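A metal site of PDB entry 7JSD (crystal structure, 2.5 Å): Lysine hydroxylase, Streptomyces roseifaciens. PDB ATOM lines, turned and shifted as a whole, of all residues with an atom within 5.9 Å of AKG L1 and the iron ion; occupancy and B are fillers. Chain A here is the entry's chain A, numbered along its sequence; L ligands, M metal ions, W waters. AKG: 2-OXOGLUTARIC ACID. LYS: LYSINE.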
ATOM      1  N   LEU A 131      -8.558 -10.103 -20.967  1.00  0.00           N
ATOM      2  CA  LEU A 131      -7.562  -9.952 -19.923  1.00  0.00           C
ATOM      3  C   LEU A 131      -7.213 -11.327 -19.378  1.00  0.00           C
ATOM      4  O   LEU A 131      -8.108 -12.150 -19.158  1.00  0.00           O
ATOM      5  CB  LEU A 131      -8.067  -9.047 -18.784  1.00  0.00           C
ATOM      6  CG  LEU A 131      -7.038  -8.657 -17.719  1.00  0.00           C
ATOM      7  CD1 LEU A 131      -6.060  -7.637 -18.273  1.00  0.00           C
ATOM      8  CD2 LEU A 131      -7.721  -8.135 -16.463  1.00  0.00           C
ATOM      9  N   THR A 133      -5.303 -12.743 -16.055  1.00  0.00           N
ATOM     10  CA  THR A 133      -4.657 -12.516 -14.764  1.00  0.00           C
ATOM     11  C   THR A 133      -3.881 -13.761 -14.373  1.00  0.00           C
ATOM     12  O   THR A 133      -4.351 -14.885 -14.559  1.00  0.00           O
ATOM     13  CB  THR A 133      -5.685 -12.175 -13.692  1.00  0.00           C
ATOM     14  OG1 THR A 133      -6.657 -13.235 -13.588  1.00  0.00           O
ATOM     15  CG2 THR A 133      -6.398 -10.872 -14.017  1.00  0.00           C
ATOM     16  N   GLN A 135      -1.792 -15.192 -11.091  1.00  0.00           N
ATOM     17  CA  GLN A 135      -1.397 -15.106  -9.694  1.00  0.00           C
ATOM     18  C   GLN A 135      -0.567 -16.328  -9.331  1.00  0.00           C
ATOM     19  O   GLN A 135      -0.880 -17.445  -9.750  1.00  0.00           O
ATOM     20  CB  GLN A 135      -2.617 -15.004  -8.782  1.00  0.00           C
ATOM     21  CG  GLN A 135      -3.642 -13.979  -9.216  1.00  0.00           C
ATOM     22  CD  GLN A 135      -4.808 -13.865  -8.265  1.00  0.00           C
ATOM     23  OE1 GLN A 135      -4.721 -14.287  -7.105  1.00  0.00           O
ATOM     24  NE2 GLN A 135      -5.915 -13.300  -8.740  1.00  0.00           N
ATOM     25  N   HIS A 142      -6.911 -10.247  -6.371  1.00  0.00           N
ATOM     26  CA  HIS A 142      -7.621  -9.277  -7.204  1.00  0.00           C
ATOM     27  C   HIS A 142      -8.708  -8.696  -6.302  1.00  0.00           C
ATOM     28  O   HIS A 142      -9.761  -9.299  -6.120  1.00  0.00           O
ATOM     29  CB  HIS A 142      -8.194  -9.954  -8.451  1.00  0.00           C
ATOM     30  CG  HIS A 142      -8.636  -8.987  -9.513  1.00  0.00           C
ATOM     31  ND1 HIS A 142      -8.661  -9.324 -10.851  1.00  0.00           N
ATOM     32  CD2 HIS A 142      -9.067  -7.712  -9.440  1.00  0.00           C
ATOM     33  CE1 HIS A 142      -9.095  -8.298 -11.554  1.00  0.00           C
ATOM     34  NE2 HIS A 142      -9.341  -7.301 -10.718  1.00  0.00           N
ATOM     35  N   HIS A 145     -13.930  -5.006  -6.194  1.00  0.00           N
ATOM     36  CA  HIS A 145     -14.111  -4.051  -7.286  1.00  0.00           C
ATOM     37  C   HIS A 145     -15.430  -4.359  -7.988  1.00  0.00           C
ATOM     38  O   HIS A 145     -16.086  -5.365  -7.727  1.00  0.00           O
ATOM     39  CB  HIS A 145     -12.955  -4.118  -8.284  1.00  0.00           C
ATOM     40  CG  HIS A 145     -12.932  -5.382  -9.089  1.00  0.00           C
ATOM     41  ND1 HIS A 145     -12.287  -6.523  -8.657  1.00  0.00           N
ATOM     42  CD2 HIS A 145     -13.487  -5.693 -10.281  1.00  0.00           C
ATOM     43  CE1 HIS A 145     -12.440  -7.479  -9.563  1.00  0.00           C
ATOM     44  NE2 HIS A 145     -13.159  -6.996 -10.563  1.00  0.00           N
ATOM     45  N   TRP A 146     -15.806  -3.454  -8.882  1.00  0.00           N
ATOM     46  CA  TRP A 146     -16.797  -3.699  -9.919  1.00  0.00           C
ATOM     47  C   TRP A 146     -16.136  -3.514 -11.280  1.00  0.00           C
ATOM     48  O   TRP A 146     -15.018  -3.025 -11.385  1.00  0.00           O
ATOM     49  CB  TRP A 146     -18.004  -2.746  -9.796  1.00  0.00           C
ATOM     50  CG  TRP A 146     -18.755  -2.829  -8.505  1.00  0.00           C
ATOM     51  CD1 TRP A 146     -19.887  -3.551  -8.252  1.00  0.00           C
ATOM     52  CD2 TRP A 146     -18.431  -2.135  -7.290  1.00  0.00           C
ATOM     53  NE1 TRP A 146     -20.285  -3.361  -6.944  1.00  0.00           N
ATOM     54  CE2 TRP A 146     -19.411  -2.499  -6.333  1.00  0.00           C
ATOM     55  CE3 TRP A 146     -17.412  -1.260  -6.916  1.00  0.00           C
ATOM     56  CZ2 TRP A 146     -19.397  -2.005  -5.033  1.00  0.00           C
ATOM     57  CZ3 TRP A 146     -17.402  -0.774  -5.617  1.00  0.00           C
ATOM     58  CH2 TRP A 146     -18.390  -1.140  -4.692  1.00  0.00           C
ATOM     59  N   ASP A 147     -16.855  -3.917 -12.317  1.00  0.00           N
ATOM     60  CA  ASP A 147     -16.413  -3.699 -13.694  1.00  0.00           C
ATOM     61  C   ASP A 147     -17.254  -2.597 -14.321  1.00  0.00           C
ATOM     62  O   ASP A 147     -18.399  -2.354 -13.924  1.00  0.00           O
ATOM     63  CB  ASP A 147     -16.509  -4.980 -14.521  1.00  0.00           C
ATOM     64  CG  ASP A 147     -15.345  -5.930 -14.273  1.00  0.00           C
ATOM     65  OD1 ASP A 147     -15.169  -6.373 -13.115  1.00  0.00           O
ATOM     66  OD2 ASP A 147     -14.615  -6.232 -15.229  1.00  0.00           O
ATOM     67  N   ALA A 152     -19.153 -10.410 -17.567  1.00  0.00           N
ATOM     68  CA  ALA A 152     -17.787 -10.937 -17.605  1.00  0.00           C
ATOM     69  C   ALA A 152     -17.871 -12.435 -17.788  1.00  0.00           C
ATOM     70  O   ALA A 152     -18.536 -13.129 -17.013  1.00  0.00           O
ATOM     71  CB  ALA A 152     -17.015 -10.591 -16.323  1.00  0.00           C
ATOM     72  N   ASN A 154     -15.570 -15.673 -17.787  1.00  0.00           N
ATOM     73  CA  ASN A 154     -14.270 -15.988 -17.219  1.00  0.00           C
ATOM     74  C   ASN A 154     -13.949 -17.462 -17.402  1.00  0.00           C
ATOM     75  O   ASN A 154     -14.828 -18.323 -17.274  1.00  0.00           O
ATOM     76  CB  ASN A 154     -14.221 -15.620 -15.739  1.00  0.00           C
ATOM     77  CG  ASN A 154     -14.486 -14.138 -15.509  1.00  0.00           C
ATOM     78  OD1 ASN A 154     -13.565 -13.332 -15.433  1.00  0.00           O
ATOM     79  ND2 ASN A 154     -15.764 -13.779 -15.403  1.00  0.00           N
ATOM     80  N   VAL A 168     -13.586 -17.191  -5.796  1.00  0.00           N
ATOM     81  CA  VAL A 168     -14.265 -15.954  -6.164  1.00  0.00           C
ATOM     82  C   VAL A 168     -15.285 -15.620  -5.075  1.00  0.00           C
ATOM     83  O   VAL A 168     -16.131 -16.442  -4.736  1.00  0.00           O
ATOM     84  CB  VAL A 168     -14.942 -16.071  -7.538  1.00  0.00           C
ATOM     85  CG1 VAL A 168     -15.751 -14.825  -7.842  1.00  0.00           C
ATOM     86  CG2 VAL A 168     -13.902 -16.316  -8.611  1.00  0.00           C
ATOM     87  N   LEU A 197     -13.539 -22.743  -7.441  1.00  0.00           N
ATOM     88  CA  LEU A 197     -13.302 -23.075  -8.838  1.00  0.00           C
ATOM     89  C   LEU A 197     -12.201 -24.124  -8.951  1.00  0.00           C
ATOM     90  O   LEU A 197     -11.293 -24.175  -8.123  1.00  0.00           O
ATOM     91  CB  LEU A 197     -12.919 -21.838  -9.655  1.00  0.00           C
ATOM     92  CG  LEU A 197     -14.001 -20.774  -9.884  1.00  0.00           C
ATOM     93  CD1 LEU A 197     -13.394 -19.533 -10.520  1.00  0.00           C
ATOM     94  CD2 LEU A 197     -15.115 -21.324 -10.763  1.00  0.00           C
ATOM     95  N   TYR A 203     -17.343 -19.330 -15.745  1.00  0.00           N
ATOM     96  CA  TYR A 203     -18.477 -18.724 -15.057  1.00  0.00           C
ATOM     97  C   TYR A 203     -18.848 -17.401 -15.705  1.00  0.00           C
ATOM     98  O   TYR A 203     -18.005 -16.707 -16.270  1.00  0.00           O
ATOM     99  CB  TYR A 203     -18.202 -18.541 -13.555  1.00  0.00           C
ATOM    100  CG  TYR A 203     -17.165 -17.507 -13.172  1.00  0.00           C
ATOM    101  CD1 TYR A 203     -17.503 -16.160 -13.055  1.00  0.00           C
ATOM    102  CD2 TYR A 203     -15.866 -17.878 -12.872  1.00  0.00           C
ATOM    103  CE1 TYR A 203     -16.568 -15.222 -12.677  1.00  0.00           C
ATOM    104  CE2 TYR A 203     -14.917 -16.934 -12.497  1.00  0.00           C
ATOM    105  CZ  TYR A 203     -15.277 -15.607 -12.401  1.00  0.00           C
ATOM    106  OH  TYR A 203     -14.345 -14.665 -12.031  1.00  0.00           O
ATOM    107  N   LEU A 205     -20.526 -13.657 -14.995  1.00  0.00           N
ATOM    108  CA  LEU A 205     -20.641 -12.714 -13.890  1.00  0.00           C
ATOM    109  C   LEU A 205     -21.350 -11.455 -14.363  1.00  0.00           C
ATOM    110  O   LEU A 205     -21.016 -10.910 -15.421  1.00  0.00           O
ATOM    111  CB  LEU A 205     -19.262 -12.344 -13.331  1.00  0.00           C
ATOM    112  CG  LEU A 205     -19.228 -11.364 -12.150  1.00  0.00           C
ATOM    113  CD1 LEU A 205     -19.760 -12.016 -10.882  1.00  0.00           C
ATOM    114  CD2 LEU A 205     -17.829 -10.830 -11.945  1.00  0.00           C
ATOM    115  N   SER A 207     -20.960  -8.268 -13.776  1.00  0.00           N
ATOM    116  CA  SER A 207     -19.786  -7.672 -13.151  1.00  0.00           C
ATOM    117  C   SER A 207     -19.957  -6.199 -12.803  1.00  0.00           C
ATOM    118  O   SER A 207     -19.091  -5.653 -12.104  1.00  0.00           O
ATOM    119  CB  SER A 207     -18.581  -7.846 -14.062  1.00  0.00           C
ATOM    120  OG  SER A 207     -18.821  -7.282 -15.341  1.00  0.00           O
ATOM    121  N   HIS A 212     -17.019  -8.009  -6.459  1.00  0.00           N
ATOM    122  CA  HIS A 212     -16.349  -9.306  -6.450  1.00  0.00           C
ATOM    123  C   HIS A 212     -14.853  -9.143  -6.273  1.00  0.00           C
ATOM    124  O   HIS A 212     -14.292  -8.049  -6.444  1.00  0.00           O
ATOM    125  CB  HIS A 212     -16.648 -10.088  -7.747  1.00  0.00           C
ATOM    126  CG  HIS A 212     -16.406  -9.296  -8.992  1.00  0.00           C
ATOM    127  ND1 HIS A 212     -17.260  -8.310  -9.426  1.00  0.00           N
ATOM    128  CD2 HIS A 212     -15.392  -9.342  -9.893  1.00  0.00           C
ATOM    129  CE1 HIS A 212     -16.788  -7.790 -10.545  1.00  0.00           C
ATOM    130  NE2 HIS A 212     -15.653  -8.395 -10.847  1.00  0.00           N
ATOM    131  N   ARG A 213     -14.202 -10.248  -5.934  1.00  0.00           N
ATOM    132  CA  ARG A 213     -12.767 -10.290  -5.705  1.00  0.00           C
ATOM    133  C   ARG A 213     -12.332 -11.749  -5.712  1.00  0.00           C
ATOM    134  O   ARG A 213     -13.155 -12.665  -5.759  1.00  0.00           O
ATOM    135  CB  ARG A 213     -12.388  -9.632  -4.377  1.00  0.00           C
ATOM    136  CG  ARG A 213     -12.666 -10.504  -3.160  1.00  0.00           C
ATOM    137  CD  ARG A 213     -11.635 -10.277  -2.067  1.00  0.00           C
ATOM    138  NE  ARG A 213     -11.836 -11.182  -0.944  1.00  0.00           N
ATOM    139  CZ  ARG A 213     -11.020 -11.260   0.114  1.00  0.00           C
ATOM    140  NH1 ARG A 213      -9.954 -10.481   0.183  1.00  0.00           N
ATOM    141  NH2 ARG A 213     -11.284 -12.119   1.084  1.00  0.00           N
ATOM    142  N   THR A 214     -11.025 -11.957  -5.666  1.00  0.00           N
ATOM    143  CA  THR A 214     -10.434 -13.284  -5.504  1.00  0.00           C
ATOM    144  C   THR A 214      -9.777 -13.371  -4.133  1.00  0.00           C
ATOM    145  O   THR A 214      -9.050 -12.455  -3.737  1.00  0.00           O
ATOM    146  CB  THR A 214      -9.430 -13.596  -6.612  1.00  0.00           C
ATOM    147  OG1 THR A 214      -8.256 -12.784  -6.451  1.00  0.00           O
ATOM    148  CG2 THR A 214     -10.032 -13.333  -7.987  1.00  0.00           C
ATOM    149  N   ARG A 224      -2.650 -19.413 -10.404  1.00  0.00           N
ATOM    150  CA  ARG A 224      -4.034 -19.125 -10.768  1.00  0.00           C
ATOM    151  C   ARG A 224      -4.030 -18.278 -12.034  1.00  0.00           C
ATOM    152  O   ARG A 224      -3.546 -17.144 -12.014  1.00  0.00           O
ATOM    153  CB  ARG A 224      -4.770 -18.419  -9.638  1.00  0.00           C
ATOM    154  CG  ARG A 224      -6.247 -18.182  -9.898  1.00  0.00           C
ATOM    155  CD  ARG A 224      -6.853 -17.283  -8.821  1.00  0.00           C
ATOM    156  NE  ARG A 224      -8.308 -17.199  -8.907  1.00  0.00           N
ATOM    157  CZ  ARG A 224      -8.956 -16.318  -9.664  1.00  0.00           C
ATOM    158  NH1 ARG A 224      -8.285 -15.450 -10.419  1.00  0.00           N
ATOM    159  NH2 ARG A 224     -10.280 -16.310  -9.688  1.00  0.00           N
ATOM    160  N   MET A 226      -6.508 -16.809 -15.066  1.00  0.00           N
ATOM    161  CA  MET A 226      -7.905 -16.542 -15.398  1.00  0.00           C
ATOM    162  C   MET A 226      -7.989 -15.719 -16.669  1.00  0.00           C
ATOM    163  O   MET A 226      -7.364 -14.656 -16.776  1.00  0.00           O
ATOM    164  CB  MET A 226      -8.608 -15.799 -14.256  1.00  0.00           C
ATOM    165  CG  MET A 226     -10.056 -15.447 -14.543  1.00  0.00           C
ATOM    166  SD  MET A 226     -11.128 -16.896 -14.513  1.00  0.00           S
ATOM    167  CE  MET A 226     -10.922 -17.425 -12.807  1.00  0.00           C
ATOM    168  N   VAL A 228     -10.314 -13.391 -18.691  1.00  0.00           N
ATOM    169  CA  VAL A 228     -11.461 -12.537 -18.425  1.00  0.00           C
ATOM    170  C   VAL A 228     -11.919 -11.916 -19.734  1.00  0.00           C
ATOM    171  O   VAL A 228     -11.152 -11.202 -20.396  1.00  0.00           O
ATOM    172  CB  VAL A 228     -11.141 -11.461 -17.384  1.00  0.00           C
ATOM    173  CG1 VAL A 228     -12.378 -10.627 -17.072  1.00  0.00           C
ATOM    174  CG2 VAL A 228     -10.581 -12.103 -16.118  1.00  0.00           C
HETATM  175  C1  AKG L   1     -11.724  -9.000 -13.475  1.00  0.00           C
HETATM  176  O1  AKG L   1     -10.776  -9.246 -14.273  1.00  0.00           O
HETATM  177  O2  AKG L   1     -12.360  -7.912 -13.558  1.00  0.00           O
HETATM  178  C2  AKG L   1     -12.096 -10.015 -12.400  1.00  0.00           C
HETATM  179  O5  AKG L   1     -12.991  -9.785 -11.666  1.00  0.00           O
HETATM  180  C3  AKG L   1     -11.300 -11.313 -12.285  1.00  0.00           C
HETATM  181  C4  AKG L   1     -11.986 -12.336 -11.374  1.00  0.00           C
HETATM  182  C5  AKG L   1     -11.305 -13.694 -11.429  1.00  0.00           C
HETATM  183  O3  AKG L   1     -10.082 -13.787 -11.674  1.00  0.00           O
HETATM  184  O4  AKG L   1     -11.983 -14.737 -11.219  1.00  0.00           O
HETATM  185  N   LYS L   2     -12.444  -2.770 -13.042  1.00  0.00           N
HETATM  186  CA  LYS L   2     -11.649  -3.925 -12.637  1.00  0.00           C
HETATM  187  C   LYS L   2     -10.770  -3.596 -11.434  1.00  0.00           C
HETATM  188  O   LYS L   2     -10.074  -4.461 -10.914  1.00  0.00           O
HETATM  189  CB  LYS L   2     -10.777  -4.421 -13.804  1.00  0.00           C
HETATM  190  CG  LYS L   2     -11.545  -5.152 -14.890  1.00  0.00           C
HETATM  191  CD  LYS L   2     -10.616  -5.732 -15.929  1.00  0.00           C
HETATM  192  CE  LYS L   2     -11.279  -6.863 -16.708  1.00  0.00           C
HETATM  193  NZ  LYS L   2     -12.558  -6.435 -17.334  1.00  0.00           N
HETATM  194  OXT LYS L   2     -10.738  -2.460 -10.962  1.00  0.00           O
HETATM  195 FE    FE M   1     -14.038  -7.973 -12.339  1.00  0.00          FE
HETATM  196  O   HOH W   1      -7.983 -12.125 -11.315  1.00  0.00           O
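An oxygen (O4) of AKG L1 lies within hydrogen-bond range of the side-chain hydroxyl of Tyr 203, at 2.5 Å.
The guanidinium group of Arg 224 lies within salt-bridge range of an oxygen (O3) of AKG L1, at 2.8 Å.
The side-chain carboxylate (OD2) of Asp 147 is in salt-bridge range of a nitrogen (NZ) of LYS L2.
An oxygen (O) of LYS L2 is in hydrogen-bond range of a ring nitrogen (NE2) of His 142, at 2.9 Å.
N of LYS L2 lies within hydrogen-bond range of O of Trp 146 (3.1 Å).
The backbone NH (N) of Asp 147 is in hydrogen-bond range of the backbone carbonyl oxygen (O) of Ser 207, 2.8 Å away.
The backbone carbonyl oxygen (O) of Tyr 203 sits at hydrogen-bond distance from the backbone NH (N) of Asn 154.
The backbone carbonyl oxygen (O) of Gln 135 is in hydrogen-bond range of the backbone NH (N) of Arg 224, 2.7 Å away.
The backbone carbonyl oxygen of Met 226 lies within hydrogen-bond range of the backbone NH of Thr 133, 2.9 Å away.
The side-chain hydroxyl (OG1) of Thr 214 sits at hydrogen-bond distance from the backbone NH (N) of His 142 (2.9 Å).
N of Val 228 is in hydrogen-bond range of O of Leu 131 (2.6 Å).
NE2 of Gln 135 is in hydrogen-bond range of OG1 of Thr 214.
Merely in contact with AKG L1: Met 226 (3.3 Å), His 142 (3.3 Å), Val 228 (3.4 Å), Val 168 (3.6 Å), Thr 214 (3.7 Å), Leu 131 (3.9 Å) and Thr 133 (3.96 Å).
Hydrophobic or aromatic side chains within 4 Å of AKG L1: Leu 131, His 142, His 145, Val 168, Tyr 203, His 212, Met 226 and Val 228.
12 residues have an atom within 4 Å of AKG L1: Leu 131, Thr 133, His 142, His 145, Asp 147, Val 168, Tyr 203, His 212, Thr 214, Arg 224, Met 226 and Val 228.
Three residues have an atom within 4 Å of the iron ion: His 145, Asp 147 and His 212.
The nearest printed residue that does not touch the iron ion is Leu 205 (4.8 Å).
The iron ion is bound by O2 of AKG L1, OD1 of Asp 147, O5 of AKG L1, NE2 of His 145 and NE2 of His 212.
The iron ion has five donor atoms within binding distance.
Water W1 lies within hydrogen-bond range of an oxygen (O3) of AKG L1, the side-chain hydroxyl of Thr 133, a ring nitrogen (ND1) of His 142 and the guanidinium group of Arg 224.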
